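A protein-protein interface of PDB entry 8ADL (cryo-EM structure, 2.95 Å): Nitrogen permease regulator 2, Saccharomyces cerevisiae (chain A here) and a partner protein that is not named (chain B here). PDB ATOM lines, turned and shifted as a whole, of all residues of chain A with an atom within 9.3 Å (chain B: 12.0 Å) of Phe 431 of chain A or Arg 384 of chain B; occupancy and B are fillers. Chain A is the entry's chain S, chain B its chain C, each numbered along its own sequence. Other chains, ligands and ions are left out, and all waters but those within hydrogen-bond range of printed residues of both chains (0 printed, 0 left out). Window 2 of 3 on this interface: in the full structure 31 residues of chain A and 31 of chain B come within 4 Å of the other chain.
Printed residues of chain B within 4 Å of Ser 336 of chain A: Arg 385.
Glu 342 of chain A touches none of the printed residues of chain B.
Val 343 of chain A touches none of the printed residues of chain B.
Of chain B, only Arg 384 (3.5 Å) comes within 4 Å of Phe 431 of chain A.
Of the printed residues of chain B, Thr 434 of chain A touches Glu 388.
Printed residues of chain A within 4 Å of Phe 383 of chain B: Leu 432.
Of the printed residues of chain A, Arg 384 of chain B touches Phe 431 and Leu 432.
Printed residues of chain A within 4 Å of Arg 385 of chain B: Ser 336 and Leu 432.
Of the printed residues of chain A, Glu 388 of chain B touches Gln 335 (3.7 Å) and Thr 434 (2.4 Å).
The nearest residue of chain B that does not touch Phe 431 of chain A is Phe 383 of chain B (4.1 Å).
The nearest residue of chain A that does not touch Arg 384 of chain B is Pro 433 of chain A (5.9 Å).
Glu 388 of chain B touches Gln 335 of chain A.
Phe 431 of chain A touches Arg 384 of chain B (CA to O, 3.5 Å).
Leu 432 of chain A touches Phe 383 of chain B (CG to O, 3.9 Å).
Arg 385 of chain B touches Leu 432 of chain A (NE to CD1, 3.7 Å).
OG1 of Thr 434 of chain A sits at hydrogen-bond distance from OE1 of Glu 388 of chain B.
O of Arg 384 of chain B lies within hydrogen-bond range of N of Leu 432 of chain A (2.7 Å).
The side-chain hydroxyl of Ser 336 of chain A lies within hydrogen-bond range of the guanidinium group of Arg 385 of chain B.
O of Gln 335 of chain A lies within hydrogen-bond range of OG1 of Thr 339 of chain A (3.0 Å).
Of the 6 printed residues of chain B, 4 touch a printed residue of chain A.
Of the 16 printed residues of chain A, 5 touch a printed residue of chain B.
Printed residues of chain A that touch a printed residue of chain B: Gln 335, Ser 336, Phe 431, Leu 432 and Thr 434.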
ATOM      1  N   GLN A 335     -18.813  27.634  22.123  1.00  0.00           N
ATOM      2  CA  GLN A 335     -19.057  26.671  21.050  1.00  0.00           C
ATOM      3  C   GLN A 335     -20.418  26.903  20.407  1.00  0.00           C
ATOM      4  O   GLN A 335     -20.545  26.884  19.178  1.00  0.00           O
ATOM      5  CB  GLN A 335     -18.970  25.244  21.592  1.00  0.00           C
ATOM      6  CG  GLN A 335     -17.587  24.810  22.042  1.00  0.00           C
ATOM      7  CD  GLN A 335     -17.511  23.321  22.330  1.00  0.00           C
ATOM      8  OE1 GLN A 335     -17.897  22.865  23.405  1.00  0.00           O
ATOM      9  NE2 GLN A 335     -17.013  22.558  21.366  1.00  0.00           N
ATOM     10  N   SER A 336     -21.447  27.124  21.225  1.00  0.00           N
ATOM     11  CA  SER A 336     -22.784  27.360  20.698  1.00  0.00           C
ATOM     12  C   SER A 336     -22.945  28.755  20.101  1.00  0.00           C
ATOM     13  O   SER A 336     -23.930  28.996  19.394  1.00  0.00           O
ATOM     14  CB  SER A 336     -23.823  27.151  21.801  1.00  0.00           C
ATOM     15  OG  SER A 336     -23.720  25.853  22.356  1.00  0.00           O
ATOM     16  N   THR A 339     -20.208  29.660  16.155  1.00  0.00           N
ATOM     17  CA  THR A 339     -20.325  28.810  14.976  1.00  0.00           C
ATOM     18  C   THR A 339     -21.508  29.235  14.112  1.00  0.00           C
ATOM     19  O   THR A 339     -22.570  29.598  14.627  1.00  0.00           O
ATOM     20  CB  THR A 339     -20.477  27.344  15.399  1.00  0.00           C
ATOM     21  OG1 THR A 339     -19.464  27.020  16.359  1.00  0.00           O
ATOM     22  CG2 THR A 339     -20.325  26.407  14.204  1.00  0.00           C
ATOM     23  N   PHE A 340     -21.305  29.210  12.791  1.00  0.00           N
ATOM     24  CA  PHE A 340     -22.391  29.434  11.850  1.00  0.00           C
ATOM     25  C   PHE A 340     -23.437  28.325  11.980  1.00  0.00           C
ATOM     26  O   PHE A 340     -23.100  27.180  12.296  1.00  0.00           O
ATOM     27  CB  PHE A 340     -21.861  29.469  10.416  1.00  0.00           C
ATOM     28  CG  PHE A 340     -20.925  30.607  10.130  1.00  0.00           C
ATOM     29  CD1 PHE A 340     -21.413  31.876   9.869  1.00  0.00           C
ATOM     30  CD2 PHE A 340     -19.555  30.398  10.096  1.00  0.00           C
ATOM     31  CE1 PHE A 340     -20.550  32.922   9.596  1.00  0.00           C
ATOM     32  CE2 PHE A 340     -18.688  31.438   9.824  1.00  0.00           C
ATOM     33  CZ  PHE A 340     -19.185  32.700   9.571  1.00  0.00           C
ATOM     34  N   PRO A 341     -24.720  28.643  11.766  1.00  0.00           N
ATOM     35  CA  PRO A 341     -25.753  27.595  11.839  1.00  0.00           C
ATOM     36  C   PRO A 341     -25.625  26.538  10.755  1.00  0.00           C
ATOM     37  O   PRO A 341     -25.955  25.372  11.003  1.00  0.00           O
ATOM     38  CB  PRO A 341     -27.062  28.384  11.703  1.00  0.00           C
ATOM     39  CG  PRO A 341     -26.675  29.622  10.969  1.00  0.00           C
ATOM     40  CD  PRO A 341     -25.298  29.963  11.457  1.00  0.00           C
ATOM     41  N   GLU A 342     -25.156  26.906   9.570  1.00  0.00           N
ATOM     42  CA  GLU A 342     -24.918  25.973   8.477  1.00  0.00           C
ATOM     43  C   GLU A 342     -23.468  26.099   8.013  1.00  0.00           C
ATOM     44  O   GLU A 342     -22.661  26.816   8.611  1.00  0.00           O
ATOM     45  CB  GLU A 342     -25.899  26.225   7.330  1.00  0.00           C
ATOM     46  CG  GLU A 342     -27.362  26.052   7.703  1.00  0.00           C
ATOM     47  CD  GLU A 342     -28.297  26.382   6.555  1.00  0.00           C
ATOM     48  OE1 GLU A 342     -27.803  26.745   5.468  1.00  0.00           O
ATOM     49  OE2 GLU A 342     -29.528  26.278   6.740  1.00  0.00           O
ATOM     50  N   VAL A 343     -23.142  25.401   6.928  1.00  0.00           N
ATOM     51  CA  VAL A 343     -21.840  25.551   6.284  1.00  0.00           C
ATOM     52  C   VAL A 343     -21.901  26.839   5.467  1.00  0.00           C
ATOM     53  O   VAL A 343     -22.401  26.855   4.341  1.00  0.00           O
ATOM     54  CB  VAL A 343     -21.485  24.342   5.415  1.00  0.00           C
ATOM     55  CG1 VAL A 343     -20.077  24.486   4.855  1.00  0.00           C
ATOM     56  CG2 VAL A 343     -21.618  23.057   6.217  1.00  0.00           C
ATOM     57  N   PHE A 431     -19.258  18.746  13.236  1.00  0.00           N
ATOM     58  CA  PHE A 431     -19.256  18.904  14.686  1.00  0.00           C
ATOM     59  C   PHE A 431     -18.869  20.330  15.061  1.00  0.00           C
ATOM     60  O   PHE A 431     -18.307  21.061  14.246  1.00  0.00           O
ATOM     61  CB  PHE A 431     -18.295  17.905  15.333  1.00  0.00           C
ATOM     62  CG  PHE A 431     -18.760  16.479  15.248  1.00  0.00           C
ATOM     63  CD1 PHE A 431     -20.100  16.165  15.401  1.00  0.00           C
ATOM     64  CD2 PHE A 431     -17.856  15.455  15.014  1.00  0.00           C
ATOM     65  CE1 PHE A 431     -20.533  14.854  15.322  1.00  0.00           C
ATOM     66  CE2 PHE A 431     -18.281  14.141  14.934  1.00  0.00           C
ATOM     67  CZ  PHE A 431     -19.622  13.841  15.089  1.00  0.00           C
ATOM     68  N   LEU A 432     -19.179  20.725  16.294  1.00  0.00           N
ATOM     69  CA  LEU A 432     -18.770  22.037  16.765  1.00  0.00           C
ATOM     70  C   LEU A 432     -17.260  22.073  17.001  1.00  0.00           C
ATOM     71  O   LEU A 432     -16.641  21.037  17.263  1.00  0.00           O
ATOM     72  CB  LEU A 432     -19.509  22.391  18.055  1.00  0.00           C
ATOM     73  CG  LEU A 432     -20.978  22.796  17.897  1.00  0.00           C
ATOM     74  CD1 LEU A 432     -21.574  23.226  19.230  1.00  0.00           C
ATOM     75  CD2 LEU A 432     -21.132  23.896  16.862  1.00  0.00           C
ATOM     76  N   PRO A 433     -16.640  23.249  16.872  1.00  0.00           N
ATOM     77  CA  PRO A 433     -15.219  23.384  17.224  1.00  0.00           C
ATOM     78  C   PRO A 433     -14.976  23.105  18.700  1.00  0.00           C
ATOM     79  O   PRO A 433     -15.764  23.497  19.562  1.00  0.00           O
ATOM     80  CB  PRO A 433     -14.898  24.841  16.869  1.00  0.00           C
ATOM     81  CG  PRO A 433     -16.233  25.518  16.721  1.00  0.00           C
ATOM     82  CD  PRO A 433     -17.151  24.460  16.210  1.00  0.00           C
ATOM     83  N   THR A 434     -13.875  22.413  18.983  1.00  0.00           N
ATOM     84  CA  THR A 434     -13.538  22.080  20.358  1.00  0.00           C
ATOM     85  C   THR A 434     -13.095  23.325  21.122  1.00  0.00           C
ATOM     86  O   THR A 434     -12.660  24.326  20.545  1.00  0.00           O
ATOM     87  CB  THR A 434     -12.445  21.010  20.408  1.00  0.00           C
ATOM     88  OG1 THR A 434     -12.088  20.754  21.772  1.00  0.00           O
ATOM     89  CG2 THR A 434     -11.213  21.459  19.639  1.00  0.00           C
ATOM     90  N   LYS A 463     -12.093  28.443   8.838  1.00  0.00           N
ATOM     91  CA  LYS A 463     -12.851  27.911   7.715  1.00  0.00           C
ATOM     92  C   LYS A 463     -13.257  26.469   7.983  1.00  0.00           C
ATOM     93  O   LYS A 463     -14.397  26.075   7.709  1.00  0.00           O
ATOM     94  CB  LYS A 463     -12.023  28.011   6.434  1.00  0.00           C
ATOM     95  CG  LYS A 463     -12.657  27.375   5.219  1.00  0.00           C
ATOM     96  CD  LYS A 463     -11.910  27.737   3.946  1.00  0.00           C
ATOM     97  CE  LYS A 463     -10.584  27.005   3.857  1.00  0.00           C
ATOM     98  NZ  LYS A 463      -9.897  27.254   2.561  1.00  0.00           N
ATOM     99  N   GLU A 464     -12.332  25.668   8.520  1.00  0.00           N
ATOM    100  CA  GLU A 464     -12.636  24.272   8.808  1.00  0.00           C
ATOM    101  C   GLU A 464     -13.588  24.135   9.988  1.00  0.00           C
ATOM    102  O   GLU A 464     -14.431  23.230   9.998  1.00  0.00           O
ATOM    103  CB  GLU A 464     -11.345  23.500   9.076  1.00  0.00           C
ATOM    104  CG  GLU A 464     -10.592  23.091   7.821  1.00  0.00           C
ATOM    105  CD  GLU A 464     -11.373  22.114   6.965  1.00  0.00           C
ATOM    106  OE1 GLU A 464     -11.965  21.169   7.528  1.00  0.00           O
ATOM    107  OE2 GLU A 464     -11.393  22.290   5.729  1.00  0.00           O
ATOM    108  N   ASN A 465     -13.481  25.015  10.983  1.00  0.00           N
ATOM    109  CA  ASN A 465     -14.338  24.930  12.157  1.00  0.00           C
ATOM    110  C   ASN A 465     -15.603  25.770  12.048  1.00  0.00           C
ATOM    111  O   ASN A 465     -16.400  25.767  12.994  1.00  0.00           O
ATOM    112  CB  ASN A 465     -13.559  25.339  13.410  1.00  0.00           C
ATOM    113  CG  ASN A 465     -12.521  24.309  13.813  1.00  0.00           C
ATOM    114  OD1 ASN A 465     -11.320  24.532  13.674  1.00  0.00           O
ATOM    115  ND2 ASN A 465     -12.984  23.171  14.316  1.00  0.00           N
ATOM    116  N   ASN A 466     -15.795  26.478  10.926  1.00  0.00           N
ATOM    117  CA  ASN A 466     -17.005  27.259  10.634  1.00  0.00           C
ATOM    118  C   ASN A 466     -17.255  28.321  11.708  1.00  0.00           C
ATOM    119  O   ASN A 466     -18.340  28.414  12.285  1.00  0.00           O
ATOM    120  CB  ASN A 466     -18.222  26.345  10.457  1.00  0.00           C
ATOM    121  CG  ASN A 466     -19.206  26.872   9.434  1.00  0.00           C
ATOM    122  OD1 ASN A 466     -18.830  27.584   8.504  1.00  0.00           O
ATOM    123  ND2 ASN A 466     -20.472  26.510   9.592  1.00  0.00           N
ATOM    124  N   ILE A 467     -16.227  29.120  11.980  1.00  0.00           N
ATOM    125  CA  ILE A 467     -16.228  30.075  13.084  1.00  0.00           C
ATOM    126  C   ILE A 467     -16.432  31.479  12.531  1.00  0.00           C
ATOM    127  O   ILE A 467     -15.702  31.912  11.630  1.00  0.00           O
ATOM    128  CB  ILE A 467     -14.925  29.981  13.897  1.00  0.00           C
ATOM    129  CG1 ILE A 467     -14.903  28.689  14.716  1.00  0.00           C
ATOM    130  CG2 ILE A 467     -14.759  31.187  14.811  1.00  0.00           C
ATOM    131  CD1 ILE A 467     -13.604  28.455  15.452  1.00  0.00           C
ATOM    132  N   PHE B 383     -24.919  22.073  15.306  1.00  0.00           N
ATOM    133  CA  PHE B 383     -24.184  20.829  15.106  1.00  0.00           C
ATOM    134  C   PHE B 383     -23.921  20.129  16.435  1.00  0.00           C
ATOM    135  O   PHE B 383     -24.183  20.683  17.502  1.00  0.00           O
ATOM    136  CB  PHE B 383     -22.860  21.098  14.385  1.00  0.00           C
ATOM    137  CG  PHE B 383     -23.024  21.548  12.961  1.00  0.00           C
ATOM    138  CD1 PHE B 383     -24.118  21.143  12.212  1.00  0.00           C
ATOM    139  CD2 PHE B 383     -22.081  22.375  12.370  1.00  0.00           C
ATOM    140  CE1 PHE B 383     -24.270  21.556  10.899  1.00  0.00           C
ATOM    141  CE2 PHE B 383     -22.226  22.791  11.058  1.00  0.00           C
ATOM    142  CZ  PHE B 383     -23.322  22.380  10.323  1.00  0.00           C
ATOM    143  N   ARG B 384     -23.400  18.906  16.360  1.00  0.00           N
ATOM    144  CA  ARG B 384     -23.125  18.121  17.551  1.00  0.00           C
ATOM    145  C   ARG B 384     -21.780  18.524  18.152  1.00  0.00           C
ATOM    146  O   ARG B 384     -21.044  19.352  17.608  1.00  0.00           O
ATOM    147  CB  ARG B 384     -23.163  16.628  17.231  1.00  0.00           C
ATOM    148  CG  ARG B 384     -24.388  16.185  16.455  1.00  0.00           C
ATOM    149  CD  ARG B 384     -24.334  14.697  16.154  1.00  0.00           C
ATOM    150  NE  ARG B 384     -25.466  14.260  15.347  1.00  0.00           N
ATOM    151  CZ  ARG B 384     -25.664  13.011  14.951  1.00  0.00           C
ATOM    152  NH1 ARG B 384     -24.821  12.042  15.269  1.00  0.00           N
ATOM    153  NH2 ARG B 384     -26.737  12.725  14.219  1.00  0.00           N
ATOM    154  N   ARG B 385     -21.453  17.924  19.293  1.00  0.00           N
ATOM    155  CA  ARG B 385     -20.226  18.216  20.019  1.00  0.00           C
ATOM    156  C   ARG B 385     -19.401  16.946  20.156  1.00  0.00           C
ATOM    157  O   ARG B 385     -19.939  15.881  20.481  1.00  0.00           O
ATOM    158  CB  ARG B 385     -20.539  18.802  21.399  1.00  0.00           C
ATOM    159  CG  ARG B 385     -21.032  20.238  21.354  1.00  0.00           C
ATOM    160  CD  ARG B 385     -21.300  20.790  22.744  1.00  0.00           C
ATOM    161  NE  ARG B 385     -22.028  22.052  22.690  1.00  0.00           N
ATOM    162  CZ  ARG B 385     -22.433  22.730  23.755  1.00  0.00           C
ATOM    163  NH1 ARG B 385     -22.199  22.293  24.982  1.00  0.00           N
ATOM    164  NH2 ARG B 385     -23.090  23.874  23.586  1.00  0.00           N
ATOM    165  N   LEU B 386     -18.101  17.062  19.899  1.00  0.00           N
ATOM    166  CA  LEU B 386     -17.189  15.942  20.080  1.00  0.00           C
ATOM    167  C   LEU B 386     -16.969  15.668  21.562  1.00  0.00           C
ATOM    168  O   LEU B 386     -16.944  16.588  22.383  1.00  0.00           O
ATOM    169  CB  LEU B 386     -15.854  16.234  19.394  1.00  0.00           C
ATOM    170  CG  LEU B 386     -14.943  15.039  19.101  1.00  0.00           C
ATOM    171  CD1 LEU B 386     -15.657  14.018  18.230  1.00  0.00           C
ATOM    172  CD2 LEU B 386     -13.651  15.502  18.445  1.00  0.00           C
ATOM    173  N   ARG B 387     -16.818  14.389  21.904  1.00  0.00           N
ATOM    174  CA  ARG B 387     -16.555  14.007  23.286  1.00  0.00           C
ATOM    175  C   ARG B 387     -15.132  14.397  23.667  1.00  0.00           C
ATOM    176  O   ARG B 387     -14.167  13.947  23.041  1.00  0.00           O
ATOM    177  CB  ARG B 387     -16.763  12.506  23.470  1.00  0.00           C
ATOM    178  CG  ARG B 387     -18.184  12.040  23.227  1.00  0.00           C
ATOM    179  CD  ARG B 387     -18.296  10.534  23.398  1.00  0.00           C
ATOM    180  NE  ARG B 387     -19.628  10.043  23.068  1.00  0.00           N
ATOM    181  CZ  ARG B 387     -19.983   8.766  23.093  1.00  0.00           C
ATOM    182  NH1 ARG B 387     -19.125   7.818  23.430  1.00  0.00           N
ATOM    183  NH2 ARG B 387     -21.230   8.432  22.772  1.00  0.00           N
ATOM    184  N   GLU B 388     -15.004  15.236  24.693  1.00  0.00           N
ATOM    185  CA  GLU B 388     -13.711  15.781  25.074  1.00  0.00           C
ATOM    186  C   GLU B 388     -13.689  16.040  26.572  1.00  0.00           C
ATOM    187  O   GLU B 388     -14.724  16.309  27.188  1.00  0.00           O
ATOM    188  CB  GLU B 388     -13.400  17.079  24.317  1.00  0.00           C
ATOM    189  CG  GLU B 388     -14.544  18.081  24.308  1.00  0.00           C
ATOM    190  CD  GLU B 388     -14.108  19.459  23.846  1.00  0.00           C
ATOM    191  OE1 GLU B 388     -12.887  19.722  23.821  1.00  0.00           O
ATOM    192  OE2 GLU B 388     -14.987  20.281  23.507  1.00  0.00           O
